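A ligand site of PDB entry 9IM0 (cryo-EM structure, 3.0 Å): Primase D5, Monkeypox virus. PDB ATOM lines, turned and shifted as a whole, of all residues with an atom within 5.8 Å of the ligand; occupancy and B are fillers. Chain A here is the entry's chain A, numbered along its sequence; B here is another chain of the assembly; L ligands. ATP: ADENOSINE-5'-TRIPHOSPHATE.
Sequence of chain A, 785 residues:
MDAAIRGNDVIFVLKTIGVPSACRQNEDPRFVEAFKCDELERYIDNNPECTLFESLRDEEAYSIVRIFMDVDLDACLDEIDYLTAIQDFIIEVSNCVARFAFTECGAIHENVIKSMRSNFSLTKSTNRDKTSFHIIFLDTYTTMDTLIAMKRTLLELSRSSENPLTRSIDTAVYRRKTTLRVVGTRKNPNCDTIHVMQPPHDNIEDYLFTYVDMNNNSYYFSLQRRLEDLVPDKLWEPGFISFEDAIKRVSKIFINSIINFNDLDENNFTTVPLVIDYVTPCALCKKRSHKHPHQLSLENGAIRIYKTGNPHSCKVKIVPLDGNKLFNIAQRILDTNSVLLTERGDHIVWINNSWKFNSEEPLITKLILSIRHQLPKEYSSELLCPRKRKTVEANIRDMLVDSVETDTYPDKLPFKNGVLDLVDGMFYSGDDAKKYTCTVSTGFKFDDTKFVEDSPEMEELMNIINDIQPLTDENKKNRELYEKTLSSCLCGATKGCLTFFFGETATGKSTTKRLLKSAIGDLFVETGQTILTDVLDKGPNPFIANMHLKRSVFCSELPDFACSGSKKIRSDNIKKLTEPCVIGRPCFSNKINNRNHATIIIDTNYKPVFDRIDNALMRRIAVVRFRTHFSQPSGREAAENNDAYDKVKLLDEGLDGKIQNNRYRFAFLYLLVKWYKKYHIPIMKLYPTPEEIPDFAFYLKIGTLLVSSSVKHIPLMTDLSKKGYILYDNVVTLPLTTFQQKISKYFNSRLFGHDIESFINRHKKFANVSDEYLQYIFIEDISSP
NH2 of Arg 181 lies within salt-bridge range of O1G of the ligand, 2.7 Å away. The guanidinium group (NE) of Arg 175 lies within hydrogen-bond range of a nitrogen (N1) of the ligand, 3.0 Å away. A ring nitrogen (NE2) of His 134 lies within hydrogen-bond range of an oxygen (O3G) of the ligand (3.1 Å). NZ of Lys 248 of chain B lies within salt-bridge range of O2B of the ligand. O of Ile 258 of chain B is in hydrogen-bond range of N6 of the ligand.
OG1 of Thr 179 lies within hydrogen-bond range of NH2 of Arg 175. OG of Ser 251 of chain B lies within hydrogen-bond range of O of Ile 247 of chain B, at 3.2 Å. The side-chain amino group (NZ) of Lys 248 of chain B is in salt-bridge range of the side-chain carboxylate (OD2) of Asp 72 (3.6 Å). A ring nitrogen (NE2) of His 195 sits at hydrogen-bond distance from the guanidinium group of Arg 181.
OD2 of Asp 70 sits close to O3G of the ligand, at 3.2 Å. Ser 132 touches the ligand (OG to O3G, 3.7 Å). Ala 172 touches the ligand. Ser 251 of chain B touches the ligand. Ser 257 of chain B touches the ligand (OG to N6, 3.9 Å). Phe 261 of chain B touches the ligand. Hydrophobic or aromatic side chains that line the ligand: His 134, Ala 172 and Phe 261 of chain B. Of the 21 residues printed, 11 come within 4 Å of the ligand. The nearest printed residue that does not touch the ligand is His 195 (4.1 Å).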
ATOM      1  N   ASP A  70       2.651  22.619 -19.703  1.00  0.00           N
ATOM      2  CA  ASP A  70       3.855  22.504 -18.894  1.00  0.00           C
ATOM      3  C   ASP A  70       4.834  21.658 -19.690  1.00  0.00           C
ATOM      4  O   ASP A  70       4.473  20.579 -20.168  1.00  0.00           O
ATOM      5  CB  ASP A  70       3.519  21.875 -17.510  1.00  0.00           C
ATOM      6  CG  ASP A  70       4.730  21.262 -16.791  1.00  0.00           C
ATOM      7  OD1 ASP A  70       5.867  21.218 -17.302  1.00  0.00           O
ATOM      8  OD2 ASP A  70       4.532  20.799 -15.645  1.00  0.00           O
ATOM      9  N   ASP A  72       8.558  19.813 -19.686  1.00  0.00           N
ATOM     10  CA  ASP A  72       9.723  19.337 -18.958  1.00  0.00           C
ATOM     11  C   ASP A  72      10.231  18.021 -19.534  1.00  0.00           C
ATOM     12  O   ASP A  72       9.455  17.093 -19.753  1.00  0.00           O
ATOM     13  CB  ASP A  72       9.401  19.166 -17.459  1.00  0.00           C
ATOM     14  CG  ASP A  72       8.221  18.244 -17.214  1.00  0.00           C
ATOM     15  OD1 ASP A  72       7.070  18.730 -17.287  1.00  0.00           O
ATOM     16  OD2 ASP A  72       8.441  17.039 -16.958  1.00  0.00           O
ATOM     17  N   SER A 132      11.494  22.840 -18.284  1.00  0.00           N
ATOM     18  CA  SER A 132      10.442  22.841 -17.265  1.00  0.00           C
ATOM     19  C   SER A 132       9.850  24.221 -17.082  1.00  0.00           C
ATOM     20  O   SER A 132      10.120  24.901 -16.090  1.00  0.00           O
ATOM     21  CB  SER A 132      10.988  22.309 -15.936  1.00  0.00           C
ATOM     22  OG  SER A 132       9.936  22.106 -15.002  1.00  0.00           O
ATOM     23  N   HIS A 134       6.175  26.776 -17.718  1.00  0.00           N
ATOM     24  CA  HIS A 134       4.716  26.783 -17.780  1.00  0.00           C
ATOM     25  C   HIS A 134       4.253  27.914 -18.693  1.00  0.00           C
ATOM     26  O   HIS A 134       4.723  29.056 -18.571  1.00  0.00           O
ATOM     27  CB  HIS A 134       4.112  26.958 -16.385  1.00  0.00           C
ATOM     28  CG  HIS A 134       4.374  25.805 -15.462  1.00  0.00           C
ATOM     29  ND1 HIS A 134       3.539  25.494 -14.413  1.00  0.00           N
ATOM     30  CD2 HIS A 134       5.380  24.903 -15.436  1.00  0.00           C
ATOM     31  CE1 HIS A 134       4.019  24.437 -13.773  1.00  0.00           C
ATOM     32  NE2 HIS A 134       5.139  24.062 -14.370  1.00  0.00           N
ATOM     33  N   ASP A 170       3.859  17.224 -21.342  1.00  0.00           N
ATOM     34  CA  ASP A 170       3.224  16.313 -20.397  1.00  0.00           C
ATOM     35  C   ASP A 170       1.720  16.497 -20.481  1.00  0.00           C
ATOM     36  O   ASP A 170       1.193  17.553 -20.137  1.00  0.00           O
ATOM     37  CB  ASP A 170       3.730  16.562 -18.983  1.00  0.00           C
ATOM     38  CG  ASP A 170       5.217  16.880 -18.939  1.00  0.00           C
ATOM     39  OD1 ASP A 170       5.621  17.913 -19.524  1.00  0.00           O
ATOM     40  OD2 ASP A 170       5.981  16.097 -18.337  1.00  0.00           O
ATOM     41  N   ALA A 172      -0.323  14.502 -18.755  1.00  0.00           N
ATOM     42  CA  ALA A 172      -0.905  13.996 -17.519  1.00  0.00           C
ATOM     43  C   ALA A 172      -1.479  15.086 -16.638  1.00  0.00           C
ATOM     44  O   ALA A 172      -2.196  14.780 -15.679  1.00  0.00           O
ATOM     45  CB  ALA A 172       0.149  13.200 -16.739  1.00  0.00           C
ATOM     46  N   VAL A 173      -1.187  16.361 -16.926  1.00  0.00           N
ATOM     47  CA  VAL A 173      -1.724  17.453 -16.123  1.00  0.00           C
ATOM     48  C   VAL A 173      -3.214  17.665 -16.379  1.00  0.00           C
ATOM     49  O   VAL A 173      -3.919  18.206 -15.522  1.00  0.00           O
ATOM     50  CB  VAL A 173      -0.936  18.742 -16.392  1.00  0.00           C
ATOM     51  CG1 VAL A 173      -1.126  19.214 -17.827  1.00  0.00           C
ATOM     52  CG2 VAL A 173      -1.302  19.833 -15.389  1.00  0.00           C
ATOM     53  N   ARG A 175      -6.720  16.560 -16.203  1.00  0.00           N
ATOM     54  CA  ARG A 175      -7.487  15.569 -15.457  1.00  0.00           C
ATOM     55  C   ARG A 175      -8.590  16.305 -14.694  1.00  0.00           C
ATOM     56  O   ARG A 175      -8.789  17.511 -14.878  1.00  0.00           O
ATOM     57  CB  ARG A 175      -6.580  14.768 -14.514  1.00  0.00           C
ATOM     58  CG  ARG A 175      -5.867  15.632 -13.479  1.00  0.00           C
ATOM     59  CD  ARG A 175      -4.950  14.806 -12.598  1.00  0.00           C
ATOM     60  NE  ARG A 175      -4.213  15.649 -11.659  1.00  0.00           N
ATOM     61  CZ  ARG A 175      -4.699  16.050 -10.491  1.00  0.00           C
ATOM     62  NH1 ARG A 175      -5.911  15.715 -10.088  1.00  0.00           N
ATOM     63  NH2 ARG A 175      -3.937  16.815  -9.706  1.00  0.00           N
ATOM     64  N   THR A 179      -4.240  20.152 -10.287  1.00  0.00           N
ATOM     65  CA  THR A 179      -3.439  21.015  -9.434  1.00  0.00           C
ATOM     66  C   THR A 179      -2.342  21.662 -10.275  1.00  0.00           C
ATOM     67  O   THR A 179      -1.650  20.972 -11.023  1.00  0.00           O
ATOM     68  CB  THR A 179      -2.823  20.238  -8.270  1.00  0.00           C
ATOM     69  OG1 THR A 179      -2.145  19.078  -8.770  1.00  0.00           O
ATOM     70  CG2 THR A 179      -3.903  19.813  -7.284  1.00  0.00           C
ATOM     71  N   ARG A 181       0.930  24.276  -9.635  1.00  0.00           N
ATOM     72  CA  ARG A 181       1.742  24.913  -8.592  1.00  0.00           C
ATOM     73  C   ARG A 181       1.792  26.427  -8.804  1.00  0.00           C
ATOM     74  O   ARG A 181       2.009  26.893  -9.919  1.00  0.00           O
ATOM     75  CB  ARG A 181       3.145  24.319  -8.584  1.00  0.00           C
ATOM     76  CG  ARG A 181       4.032  24.850  -7.465  1.00  0.00           C
ATOM     77  CD  ARG A 181       5.223  23.939  -7.222  1.00  0.00           C
ATOM     78  NE  ARG A 181       6.090  23.839  -8.398  1.00  0.00           N
ATOM     79  CZ  ARG A 181       7.266  23.245  -8.403  1.00  0.00           C
ATOM     80  NH1 ARG A 181       7.779  22.695  -7.312  1.00  0.00           N
ATOM     81  NH2 ARG A 181       7.968  23.200  -9.537  1.00  0.00           N
ATOM     82  N   LYS A 187       7.569  23.122  -3.794  1.00  0.00           N
ATOM     83  CA  LYS A 187       6.878  21.837  -3.687  1.00  0.00           C
ATOM     84  C   LYS A 187       6.936  21.307  -2.259  1.00  0.00           C
ATOM     85  O   LYS A 187       5.927  20.807  -1.744  1.00  0.00           O
ATOM     86  CB  LYS A 187       7.508  20.828  -4.661  1.00  0.00           C
ATOM     87  CG  LYS A 187       6.776  19.497  -4.728  1.00  0.00           C
ATOM     88  CD  LYS A 187       7.646  18.367  -4.193  1.00  0.00           C
ATOM     89  CE  LYS A 187       6.975  17.019  -4.356  1.00  0.00           C
ATOM     90  NZ  LYS A 187       7.813  15.914  -3.832  1.00  0.00           N
ATOM     91  N   HIS A 195       9.811  28.789  -8.869  1.00  0.00           N
ATOM     92  CA  HIS A 195       9.537  29.327 -10.189  1.00  0.00           C
ATOM     93  C   HIS A 195       9.929  30.796 -10.227  1.00  0.00           C
ATOM     94  O   HIS A 195       9.393  31.610  -9.465  1.00  0.00           O
ATOM     95  CB  HIS A 195       8.067  29.161 -10.568  1.00  0.00           C
ATOM     96  CG  HIS A 195       7.633  27.733 -10.722  1.00  0.00           C
ATOM     97  ND1 HIS A 195       7.970  26.974 -11.824  1.00  0.00           N
ATOM     98  CD2 HIS A 195       6.882  26.939  -9.927  1.00  0.00           C
ATOM     99  CE1 HIS A 195       7.461  25.766 -11.700  1.00  0.00           C
ATOM    100  NE2 HIS A 195       6.795  25.720 -10.556  1.00  0.00           N
ATOM    101  N   GLU B 244       9.976   8.996  -9.402  1.00  0.00           N
ATOM    102  CA  GLU B 244       9.132   9.943 -10.126  1.00  0.00           C
ATOM    103  C   GLU B 244       9.180   9.685 -11.624  1.00  0.00           C
ATOM    104  O   GLU B 244       8.146   9.734 -12.298  1.00  0.00           O
ATOM    105  CB  GLU B 244       9.552  11.376  -9.815  1.00  0.00           C
ATOM    106  CG  GLU B 244       9.183  11.845  -8.420  1.00  0.00           C
ATOM    107  CD  GLU B 244      10.242  11.511  -7.381  1.00  0.00           C
ATOM    108  OE1 GLU B 244      11.310  11.005  -7.780  1.00  0.00           O
ATOM    109  OE2 GLU B 244      10.004  11.753  -6.184  1.00  0.00           O
ATOM    110  N   ILE B 247       7.155   6.520 -12.403  1.00  0.00           N
ATOM    111  CA  ILE B 247       5.731   6.793 -12.320  1.00  0.00           C
ATOM    112  C   ILE B 247       5.277   7.618 -13.515  1.00  0.00           C
ATOM    113  O   ILE B 247       4.172   7.416 -14.049  1.00  0.00           O
ATOM    114  CB  ILE B 247       5.398   7.487 -10.983  1.00  0.00           C
ATOM    115  CG1 ILE B 247       5.568   6.502  -9.827  1.00  0.00           C
ATOM    116  CG2 ILE B 247       3.985   8.042 -10.997  1.00  0.00           C
ATOM    117  CD1 ILE B 247       4.532   5.393  -9.828  1.00  0.00           C
ATOM    118  N   LYS B 248       6.109   8.559 -13.965  1.00  0.00           N
ATOM    119  CA  LYS B 248       5.770   9.345 -15.150  1.00  0.00           C
ATOM    120  C   LYS B 248       5.664   8.467 -16.385  1.00  0.00           C
ATOM    121  O   LYS B 248       4.743   8.632 -17.197  1.00  0.00           O
ATOM    122  CB  LYS B 248       6.810  10.453 -15.359  1.00  0.00           C
ATOM    123  CG  LYS B 248       6.592  11.682 -14.482  1.00  0.00           C
ATOM    124  CD  LYS B 248       7.677  12.718 -14.712  1.00  0.00           C
ATOM    125  CE  LYS B 248       7.457  13.941 -13.843  1.00  0.00           C
ATOM    126  NZ  LYS B 248       8.540  14.946 -14.022  1.00  0.00           N
ATOM    127  N   SER B 251       2.409   6.451 -16.105  1.00  0.00           N
ATOM    128  CA  SER B 251       1.270   7.307 -16.424  1.00  0.00           C
ATOM    129  C   SER B 251       1.244   7.713 -17.892  1.00  0.00           C
ATOM    130  O   SER B 251       0.176   8.064 -18.405  1.00  0.00           O
ATOM    131  CB  SER B 251       1.274   8.543 -15.537  1.00  0.00           C
ATOM    132  OG  SER B 251       1.095   8.201 -14.178  1.00  0.00           O
ATOM    133  N   SER B 257      -6.313   8.787 -16.963  1.00  0.00           N
ATOM    134  CA  SER B 257      -5.738   9.220 -15.704  1.00  0.00           C
ATOM    135  C   SER B 257      -5.901   8.134 -14.635  1.00  0.00           C
ATOM    136  O   SER B 257      -6.608   7.146 -14.812  1.00  0.00           O
ATOM    137  CB  SER B 257      -6.399  10.516 -15.238  1.00  0.00           C
ATOM    138  OG  SER B 257      -5.947  10.880 -13.941  1.00  0.00           O
ATOM    139  N   ILE B 258      -5.219   8.339 -13.512  1.00  0.00           N
ATOM    140  CA  ILE B 258      -5.265   7.434 -12.372  1.00  0.00           C
ATOM    141  C   ILE B 258      -5.857   8.200 -11.203  1.00  0.00           C
ATOM    142  O   ILE B 258      -5.342   9.259 -10.817  1.00  0.00           O
ATOM    143  CB  ILE B 258      -3.879   6.880 -12.010  1.00  0.00           C
ATOM    144  CG1 ILE B 258      -3.092   6.547 -13.279  1.00  0.00           C
ATOM    145  CG2 ILE B 258      -4.004   5.657 -11.118  1.00  0.00           C
ATOM    146  CD1 ILE B 258      -1.819   5.755 -13.023  1.00  0.00           C
ATOM    147  N   ILE B 259      -6.941   7.670 -10.629  1.00  0.00           N
ATOM    148  CA  ILE B 259      -7.591   8.340  -9.497  1.00  0.00           C
ATOM    149  C   ILE B 259      -6.947   7.994  -8.161  1.00  0.00           C
ATOM    150  O   ILE B 259      -7.327   8.583  -7.146  1.00  0.00           O
ATOM    151  CB  ILE B 259      -9.091   7.987  -9.431  1.00  0.00           C
ATOM    152  CG1 ILE B 259      -9.277   6.484  -9.202  1.00  0.00           C
ATOM    153  CG2 ILE B 259      -9.796   8.419 -10.701  1.00  0.00           C
ATOM    154  CD1 ILE B 259     -10.714   6.094  -8.889  1.00  0.00           C
ATOM    155  N   PHE B 261      -3.489   8.113  -7.746  1.00  0.00           N
ATOM    156  CA  PHE B 261      -2.088   8.516  -7.929  1.00  0.00           C
ATOM    157  C   PHE B 261      -1.465   8.978  -6.615  1.00  0.00           C
ATOM    158  O   PHE B 261      -0.297   8.671  -6.349  1.00  0.00           O
ATOM    159  CB  PHE B 261      -1.999   9.621  -8.979  1.00  0.00           C
ATOM    160  CG  PHE B 261      -0.658  10.300  -9.037  1.00  0.00           C
ATOM    161  CD1 PHE B 261       0.426   9.661  -9.623  1.00  0.00           C
ATOM    162  CD2 PHE B 261      -0.487  11.572  -8.515  1.00  0.00           C
ATOM    163  CE1 PHE B 261       1.659  10.283  -9.671  1.00  0.00           C
ATOM    164  CE2 PHE B 261       0.744  12.188  -8.570  1.00  0.00           C
ATOM    165  CZ  PHE B 261       1.813  11.542  -9.145  1.00  0.00           C
ATOM    166  N   ASN B 262      -2.214   9.705  -5.789  1.00  0.00           N
ATOM    167  CA  ASN B 262      -1.652  10.241  -4.555  1.00  0.00           C
ATOM    168  C   ASN B 262      -1.307   9.139  -3.566  1.00  0.00           C
ATOM    169  O   ASN B 262      -0.400   9.324  -2.740  1.00  0.00           O
ATOM    170  CB  ASN B 262      -2.639  11.230  -3.922  1.00  0.00           C
ATOM    171  CG  ASN B 262      -2.776  12.512  -4.721  1.00  0.00           C
ATOM    172  OD1 ASN B 262      -1.787  13.047  -5.220  1.00  0.00           O
ATOM    173  ND2 ASN B 262      -4.005  13.000  -4.852  1.00  0.00           N
HETATM  174  PG  ATP L   1       5.801  21.123 -12.217  1.00  0.00           P
HETATM  175  O1G ATP L   1       6.278  21.678 -10.922  1.00  0.00           O
HETATM  176  O2G ATP L   1       4.335  21.446 -12.515  1.00  0.00           O
HETATM  177  O3G ATP L   1       6.653  21.530 -13.426  1.00  0.00           O
HETATM  178  PB  ATP L   1       6.794  18.323 -11.709  1.00  0.00           P
HETATM  179  O1B ATP L   1       7.629  18.725 -10.564  1.00  0.00           O
HETATM  180  O2B ATP L   1       7.571  17.811 -12.925  1.00  0.00           O
HETATM  181  O3B ATP L   1       5.853  19.508 -12.215  1.00  0.00           O
HETATM  182  PA  ATP L   1       4.907  16.764 -10.021  1.00  0.00           P
HETATM  183  O1A ATP L   1       4.139  17.885  -9.452  1.00  0.00           O
HETATM  184  O2A ATP L   1       5.899  16.099  -9.067  1.00  0.00           O
HETATM  185  O3A ATP L   1       5.722  17.202 -11.323  1.00  0.00           O
HETATM  186  O5' ATP L   1       3.932  15.653 -10.575  1.00  0.00           O
HETATM  187  C5' ATP L   1       4.352  14.276 -10.723  1.00  0.00           C
HETATM  188  C4' ATP L   1       3.967  13.823 -12.100  1.00  0.00           C
HETATM  189  O4' ATP L   1       3.060  12.702 -12.010  1.00  0.00           O
HETATM  190  C3' ATP L   1       3.202  14.830 -12.934  1.00  0.00           C
HETATM  191  O3' ATP L   1       4.078  15.751 -13.564  1.00  0.00           O
HETATM  192  C2' ATP L   1       2.490  13.943 -13.963  1.00  0.00           C
HETATM  193  O2' ATP L   1       3.298  13.745 -15.123  1.00  0.00           O
HETATM  194  C1' ATP L   1       2.326  12.611 -13.209  1.00  0.00           C
HETATM  195  N9  ATP L   1       0.941  12.251 -12.894  1.00  0.00           N
HETATM  196  C8  ATP L   1       0.270  11.148 -13.331  1.00  0.00           C
HETATM  197  N7  ATP L   1      -0.965  11.054 -12.891  1.00  0.00           N
HETATM  198  C5  ATP L   1      -1.111  12.193 -12.106  1.00  0.00           C
HETATM  199  C6  ATP L   1      -2.194  12.696 -11.361  1.00  0.00           C
HETATM  200  N6  ATP L   1      -3.391  12.087 -11.268  1.00  0.00           N
HETATM  201  N1  ATP L   1      -2.009  13.853 -10.685  1.00  0.00           N
HETATM  202  C2  ATP L   1      -0.826  14.466 -10.776  1.00  0.00           C
HETATM  203  N3  ATP L   1       0.265  14.087 -11.440  1.00  0.00           N
HETATM  204  C4  ATP L   1       0.053  12.932 -12.097  1.00  0.00           C
